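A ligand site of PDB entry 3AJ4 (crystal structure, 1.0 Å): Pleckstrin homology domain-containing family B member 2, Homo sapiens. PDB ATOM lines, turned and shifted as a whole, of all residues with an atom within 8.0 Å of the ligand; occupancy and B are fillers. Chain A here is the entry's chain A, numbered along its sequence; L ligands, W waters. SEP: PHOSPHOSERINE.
OG of Ser 15 lies within hydrogen-bond range of O3P of the ligand.
The backbone NH (N) of Thr 16 lies within hydrogen-bond range of an oxygen (OXT) of the ligand (2.9 Å).
An oxygen (O) of the ligand is in salt-bridge range of the guanidinium group (NH2) of Arg 13.
NZ of Lys 22 lies within salt-bridge range of O2P of the ligand.
OG1 of Thr 16 lies within hydrogen-bond range of OXT of the ligand (3.2 Å).
The backbone NH (N) of Ile 17 lies within hydrogen-bond range of an oxygen (O3P) of the ligand (3.1 Å).
An oxygen (O2P) of the ligand lies within salt-bridge range of the guanidinium group (NE) of Arg 20 (2.8 Å).
The backbone NH (N) of Leu 18 lies within hydrogen-bond range of an oxygen (O3P) of the ligand, 2.8 Å away.
OE2 of Glu 46 lies within salt-bridge range of N of the ligand.
Water W2 lies within hydrogen-bond range of a nitrogen (N) of the ligand and the side-chain amino group (NZ) of Lys 22.
Water W3 bridges an oxygen (O1P) of the ligand and the guanidinium group (NH2) of Arg 20.
Water W1 lies within hydrogen-bond range of the side-chain carboxylate (OE1) of Glu 46 (2.8 Å) and a nitrogen (N) of the ligand (3.3 Å).
The side-chain amide oxygen of Asn 24 lies within hydrogen-bond range of the guanidinium group of Arg 13 (2.9 Å).
N of Glu 46 is in hydrogen-bond range of O of Tyr 36 (2.9 Å).
The backbone NH (N) of Ser 15 is in hydrogen-bond range of the backbone carbonyl oxygen (O) of Arg 20.
OG of Ser 15 lies within hydrogen-bond range of N of Lys 19, 3.0 Å away.
The backbone NH (N) of Arg 13 lies within hydrogen-bond range of the backbone carbonyl oxygen (O) of Lys 22 (2.8 Å).
Hydrophobic or aromatic side chains within 4 Å of the ligand: Ile 17 and Leu 18.
The nearest printed residue that does not touch the ligand is Lys 19 (4.3 Å).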
ATOM      1  N   ARG A  13       8.780   2.058 -31.110  1.00  0.00           N
ATOM      2  CA  ARG A  13       9.376   3.383 -31.134  1.00  0.00           C
ATOM      3  C   ARG A  13      10.819   3.279 -30.717  1.00  0.00           C
ATOM      4  O   ARG A  13      11.129   2.534 -29.770  1.00  0.00           O
ATOM      5  CB  ARG A  13       8.614   4.327 -30.205  1.00  0.00           C
ATOM      6  CG  ARG A  13       9.154   5.744 -30.155  1.00  0.00           C
ATOM      7  CD  ARG A  13       8.315   6.637 -29.266  1.00  0.00           C
ATOM      8  NE  ARG A  13       8.221   6.159 -27.905  1.00  0.00           N
ATOM      9  CZ  ARG A  13       9.160   6.283 -26.982  1.00  0.00           C
ATOM     10  NH1 ARG A  13      10.260   6.968 -27.205  1.00  0.00           N
ATOM     11  NH2 ARG A  13       8.968   5.682 -25.806  1.00  0.00           N
ATOM     12  N   GLN A  14      11.720   3.981 -31.385  1.00  0.00           N
ATOM     13  CA  GLN A  14      13.105   4.034 -30.911  1.00  0.00           C
ATOM     14  C   GLN A  14      13.195   4.987 -29.772  1.00  0.00           C
ATOM     15  O   GLN A  14      12.785   6.151 -29.860  1.00  0.00           O
ATOM     16  CB  GLN A  14      14.120   4.457 -31.944  1.00  0.00           C
ATOM     17  CG  GLN A  14      14.672   3.264 -32.532  1.00  0.00           C
ATOM     18  CD  GLN A  14      15.775   3.471 -33.520  1.00  0.00           C
ATOM     19  OE1 GLN A  14      15.940   4.523 -34.108  1.00  0.00           O
ATOM     20  NE2 GLN A  14      16.544   2.433 -33.739  1.00  0.00           N
ATOM     21  N   SER A  15      13.775   4.483 -28.699  1.00  0.00           N
ATOM     22  CA  SER A  15      13.802   5.236 -27.465  1.00  0.00           C
ATOM     23  C   SER A  15      14.827   6.386 -27.496  1.00  0.00           C
ATOM     24  O   SER A  15      15.705   6.452 -28.313  1.00  0.00           O
ATOM     25  CB  SER A  15      14.061   4.300 -26.316  1.00  0.00           C
ATOM     26  OG  SER A  15      15.418   3.941 -26.264  1.00  0.00           O
ATOM     27  N   THR A  16      14.661   7.292 -26.540  1.00  0.00           N
ATOM     28  CA  THR A  16      15.356   8.579 -26.550  1.00  0.00           C
ATOM     29  C   THR A  16      16.690   8.590 -25.826  1.00  0.00           C
ATOM     30  O   THR A  16      17.416   9.583 -25.963  1.00  0.00           O
ATOM     31  CB  THR A  16      14.480   9.717 -25.983  1.00  0.00           C
ATOM     32  OG1 THR A  16      14.205   9.461 -24.623  1.00  0.00           O
ATOM     33  CG2 THR A  16      13.198   9.916 -26.798  1.00  0.00           C
ATOM     34  N   ILE A  17      17.029   7.532 -25.068  1.00  0.00           N
ATOM     35  CA  ILE A  17      18.293   7.432 -24.361  1.00  0.00           C
ATOM     36  C   ILE A  17      19.101   6.306 -24.954  1.00  0.00           C
ATOM     37  O   ILE A  17      20.233   6.494 -25.435  1.00  0.00           O
ATOM     38  CB  ILE A  17      18.109   7.292 -22.820  1.00  0.00           C
ATOM     39  CG1 ILE A  17      17.374   8.508 -22.256  1.00  0.00           C
ATOM     40  CG2 ILE A  17      19.450   7.082 -22.172  1.00  0.00           C
ATOM     41  CD1 ILE A  17      16.981   8.367 -20.781  1.00  0.00           C
ATOM     42  N   LEU A  18      18.520   5.109 -24.967  1.00  0.00           N
ATOM     43  CA  LEU A  18      19.199   3.913 -25.426  1.00  0.00           C
ATOM     44  C   LEU A  18      19.008   3.683 -26.960  1.00  0.00           C
ATOM     45  O   LEU A  18      19.713   2.866 -27.518  1.00  0.00           O
ATOM     46  CB  LEU A  18      18.648   2.695 -24.683  1.00  0.00           C
ATOM     47  CG  LEU A  18      18.845   2.746 -23.166  1.00  0.00           C
ATOM     48  CD1 LEU A  18      18.172   1.593 -22.505  1.00  0.00           C
ATOM     49  CD2 LEU A  18      20.317   2.817 -22.780  1.00  0.00           C
ATOM     50  N   LYS A  19      18.081   4.365 -27.607  1.00  0.00           N
ATOM     51  CA  LYS A  19      17.746   4.161 -29.025  1.00  0.00           C
ATOM     52  C   LYS A  19      17.296   2.728 -29.283  1.00  0.00           C
ATOM     53  O   LYS A  19      17.518   2.203 -30.342  1.00  0.00           O
ATOM     54  CB  LYS A  19      18.933   4.503 -29.938  1.00  0.00           C
ATOM     55  CG  LYS A  19      18.508   4.985 -31.331  1.00  0.00           C
ATOM     56  CD  LYS A  19      19.593   5.704 -32.076  1.00  0.00           C
ATOM     57  CE  LYS A  19      19.367   5.849 -33.543  1.00  0.00           C
ATOM     58  NZ  LYS A  19      18.067   6.173 -34.135  1.00  0.00           N
ATOM     59  N   ARG A  20      16.695   2.076 -28.276  1.00  0.00           N
ATOM     60  CA  ARG A  20      16.180   0.723 -28.451  1.00  0.00           C
ATOM     61  C   ARG A  20      14.799   0.758 -29.028  1.00  0.00           C
ATOM     62  O   ARG A  20      13.977   1.623 -28.720  1.00  0.00           O
ATOM     63  CB  ARG A  20      16.177  -0.034 -27.099  1.00  0.00           C
ATOM     64  CG  ARG A  20      15.220   0.499 -26.044  1.00  0.00           C
ATOM     65  CD  ARG A  20      15.443  -0.199 -24.730  1.00  0.00           C
ATOM     66  NE  ARG A  20      14.632   0.339 -23.655  1.00  0.00           N
ATOM     67  CZ  ARG A  20      13.557  -0.230 -23.151  1.00  0.00           C
ATOM     68  NH1 ARG A  20      13.011  -1.332 -23.642  1.00  0.00           N
ATOM     69  NH2 ARG A  20      12.975   0.345 -22.110  1.00  0.00           N
ATOM     70  N   TRP A  21      14.483  -0.225 -29.895  1.00  0.00           N
ATOM     71  CA  TRP A  21      13.115  -0.388 -30.383  1.00  0.00           C
ATOM     72  C   TRP A  21      12.280  -0.999 -29.303  1.00  0.00           C
ATOM     73  O   TRP A  21      12.550  -2.129 -28.862  1.00  0.00           O
ATOM     74  CB  TRP A  21      13.111  -1.295 -31.625  1.00  0.00           C
ATOM     75  CG  TRP A  21      13.598  -0.639 -32.851  1.00  0.00           C
ATOM     76  CD1 TRP A  21      14.736  -0.912 -33.536  1.00  0.00           C
ATOM     77  CD2 TRP A  21      12.906   0.373 -33.577  1.00  0.00           C
ATOM     78  NE1 TRP A  21      14.818  -0.110 -34.635  1.00  0.00           N
ATOM     79  CE2 TRP A  21      13.702   0.698 -34.687  1.00  0.00           C
ATOM     80  CE3 TRP A  21      11.715   1.071 -33.388  1.00  0.00           C
ATOM     81  CZ2 TRP A  21      13.360   1.683 -35.615  1.00  0.00           C
ATOM     82  CZ3 TRP A  21      11.366   2.050 -34.297  1.00  0.00           C
ATOM     83  CH2 TRP A  21      12.175   2.350 -35.394  1.00  0.00           C
ATOM     84  N   LYS A  22      11.238  -0.296 -28.869  1.00  0.00           N
ATOM     85  CA  LYS A  22      10.375  -0.795 -27.807  1.00  0.00           C
ATOM     86  C   LYS A  22       8.922  -0.555 -28.143  1.00  0.00           C
ATOM     87  O   LYS A  22       8.538   0.421 -28.790  1.00  0.00           O
ATOM     88  CB  LYS A  22      10.773  -0.233 -26.472  1.00  0.00           C
ATOM     89  CG  LYS A  22      10.591   1.247 -26.358  1.00  0.00           C
ATOM     90  CD  LYS A  22      11.249   1.639 -25.029  1.00  0.00           C
ATOM     91  CE  LYS A  22      10.969   3.054 -24.658  1.00  0.00           C
ATOM     92  NZ  LYS A  22      11.583   3.315 -23.264  1.00  0.00           N
ATOM     93  N   LYS A  23       8.084  -1.476 -27.684  1.00  0.00           N
ATOM     94  CA  LYS A  23       6.650  -1.406 -27.930  1.00  0.00           C
ATOM     95  C   LYS A  23       6.073  -0.200 -27.162  1.00  0.00           C
ATOM     96  O   LYS A  23       6.387   0.029 -25.997  1.00  0.00           O
ATOM     97  CB  LYS A  23       5.980  -2.710 -27.503  1.00  0.00           C
ATOM     98  CG  LYS A  23       4.531  -2.898 -27.948  1.00  0.00           C
ATOM     99  CD  LYS A  23       3.853  -4.304 -27.642  1.00  0.00           C
ATOM    100  CE  LYS A  23       3.140  -4.951 -28.815  1.00  0.00           C
ATOM    101  NZ  LYS A  23       4.260  -5.647 -29.602  1.00  0.00           N
ATOM    102  N   ASN A  24       5.212   0.565 -27.818  1.00  0.00           N
ATOM    103  CA  ASN A  24       4.394   1.568 -27.159  1.00  0.00           C
ATOM    104  C   ASN A  24       2.978   1.531 -27.767  1.00  0.00           C
ATOM    105  O   ASN A  24       2.782   1.124 -28.893  1.00  0.00           O
ATOM    106  CB  ASN A  24       4.966   2.980 -27.332  1.00  0.00           C
ATOM    107  CG  ASN A  24       6.000   3.460 -26.332  1.00  0.00           C
ATOM    108  OD1 ASN A  24       6.327   4.670 -26.382  1.00  0.00           O
ATOM    109  ND2 ASN A  24       6.513   2.621 -25.453  1.00  0.00           N
ATOM    110  N   TYR A  36       1.580   8.593 -26.664  1.00  0.00           N
ATOM    111  CA  TYR A  36       2.129   7.235 -26.546  1.00  0.00           C
ATOM    112  C   TYR A  36       2.431   6.900 -25.119  1.00  0.00           C
ATOM    113  O   TYR A  36       2.911   7.731 -24.318  1.00  0.00           O
ATOM    114  CB  TYR A  36       3.299   6.980 -27.508  1.00  0.00           C
ATOM    115  CG  TYR A  36       4.278   8.085 -27.706  1.00  0.00           C
ATOM    116  CD1 TYR A  36       5.534   8.034 -27.120  1.00  0.00           C
ATOM    117  CD2 TYR A  36       3.990   9.166 -28.528  1.00  0.00           C
ATOM    118  CE1 TYR A  36       6.505   9.011 -27.337  1.00  0.00           C
ATOM    119  CE2 TYR A  36       4.950  10.146 -28.778  1.00  0.00           C
ATOM    120  CZ  TYR A  36       6.215  10.036 -28.194  1.00  0.00           C
ATOM    121  OH  TYR A  36       7.148  10.993 -28.462  1.00  0.00           O
ATOM    122  N   ASP A  38       3.598   3.387 -22.384  1.00  0.00           N
ATOM    123  CA  ASP A  38       4.379   2.158 -22.294  1.00  0.00           C
ATOM    124  C   ASP A  38       3.560   0.956 -22.778  1.00  0.00           C
ATOM    125  O   ASP A  38       4.116   0.049 -23.375  1.00  0.00           O
ATOM    126  CB  ASP A  38       4.809   1.788 -20.857  1.00  0.00           C
ATOM    127  CG  ASP A  38       5.724   2.727 -20.206  1.00  0.00           C
ATOM    128  OD1 ASP A  38       6.037   2.434 -19.035  1.00  0.00           O
ATOM    129  OD2 ASP A  38       6.137   3.718 -20.795  1.00  0.00           O
ATOM    130  N   ILE A  45       2.116   7.298 -19.241  1.00  0.00           N
ATOM    131  CA  ILE A  45       2.272   8.166 -20.317  1.00  0.00           C
ATOM    132  C   ILE A  45       3.764   8.410 -20.514  1.00  0.00           C
ATOM    133  O   ILE A  45       4.550   8.637 -19.588  1.00  0.00           O
ATOM    134  CB  ILE A  45       1.378   9.411 -20.094  1.00  0.00           C
ATOM    135  CG1 ILE A  45       1.211  10.093 -21.402  1.00  0.00           C
ATOM    136  CG2 ILE A  45       1.957  10.309 -18.990  1.00  0.00           C
ATOM    137  CD1 ILE A  45       0.399  11.275 -21.425  1.00  0.00           C
ATOM    138  N   GLU A  46       4.166   8.370 -21.757  1.00  0.00           N
ATOM    139  CA  GLU A  46       5.540   8.660 -22.156  1.00  0.00           C
ATOM    140  C   GLU A  46       5.649  10.063 -22.703  1.00  0.00           C
ATOM    141  O   GLU A  46       6.412  10.879 -22.178  1.00  0.00           O
ATOM    142  CB  GLU A  46       6.068   7.604 -23.121  1.00  0.00           C
ATOM    143  CG  GLU A  46       7.520   7.897 -23.575  1.00  0.00           C
ATOM    144  CD  GLU A  46       8.490   7.767 -22.446  1.00  0.00           C
ATOM    145  OE1 GLU A  46       8.282   6.878 -21.581  1.00  0.00           O
ATOM    146  OE2 GLU A  46       9.461   8.550 -22.375  1.00  0.00           O
ATOM    147  N   ASP A  47       4.929  10.346 -23.785  1.00  0.00           N
ATOM    148  CA  ASP A  47       5.060  11.662 -24.384  1.00  0.00           C
ATOM    149  C   ASP A  47       3.951  11.818 -25.380  1.00  0.00           C
ATOM    150  O   ASP A  47       3.078  10.973 -25.561  1.00  0.00           O
ATOM    151  CB  ASP A  47       6.457  11.848 -25.018  1.00  0.00           C
ATOM    152  CG  ASP A  47       7.084  13.216 -24.738  1.00  0.00           C
ATOM    153  OD1 ASP A  47       6.377  14.246 -24.807  1.00  0.00           O
ATOM    154  OD2 ASP A  47       8.320  13.185 -24.491  1.00  0.00           O
ATOM    155  N   LYS A  87      13.059  17.210 -32.688  1.00  0.00           N
ATOM    156  CA  LYS A  87      12.714  15.889 -32.233  1.00  0.00           C
ATOM    157  C   LYS A  87      12.248  15.069 -33.434  1.00  0.00           C
ATOM    158  O   LYS A  87      11.369  15.488 -34.186  1.00  0.00           O
ATOM    159  CB  LYS A  87      11.600  15.947 -31.202  1.00  0.00           C
ATOM    160  CG  LYS A  87      11.200  14.596 -30.623  1.00  0.00           C
ATOM    161  CD  LYS A  87      10.265  14.692 -29.440  1.00  0.00           C
ATOM    162  CE  LYS A  87       9.980  13.413 -28.746  1.00  0.00           C
ATOM    163  NZ  LYS A  87      11.142  12.731 -28.163  1.00  0.00           N
HETATM  164  N   SEP L   1      11.779   7.148 -21.533  1.00  0.00           N
HETATM  165  CA  SEP L   1      12.540   7.382 -22.785  1.00  0.00           C
HETATM  166  CB  SEP L   1      13.920   6.767 -22.694  1.00  0.00           C
HETATM  167  OG  SEP L   1      13.772   5.352 -22.732  1.00  0.00           O
HETATM  168  C   SEP L   1      11.761   6.767 -23.946  1.00  0.00           C
HETATM  169  O   SEP L   1      10.816   6.035 -23.693  1.00  0.00           O
HETATM  170  OXT SEP L   1      12.172   7.060 -25.085  1.00  0.00           O
HETATM  171  P   SEP L   1      15.054   4.399 -22.758  1.00  0.00           P
HETATM  172  O1P SEP L   1      15.709   4.548 -21.412  1.00  0.00           O
HETATM  173  O2P SEP L   1      14.392   3.065 -23.030  1.00  0.00           O
HETATM  174  O3P SEP L   1      15.949   4.866 -23.894  1.00  0.00           O
HETATM  175  O   HOH W   1       9.543   7.507 -19.175  1.00  0.00           O
HETATM  176  O   HOH W   2      10.956   4.624 -20.718  1.00  0.00           O
HETATM  177  O   HOH W   3      14.835   1.922 -20.266  1.00  0.00           O
HETATM  178  O   HOH W   4      17.960   4.389 -19.880  1.00  0.00           O
HETATM  179  O   HOH W   5      14.503   5.589 -19.278  1.00  0.00           O
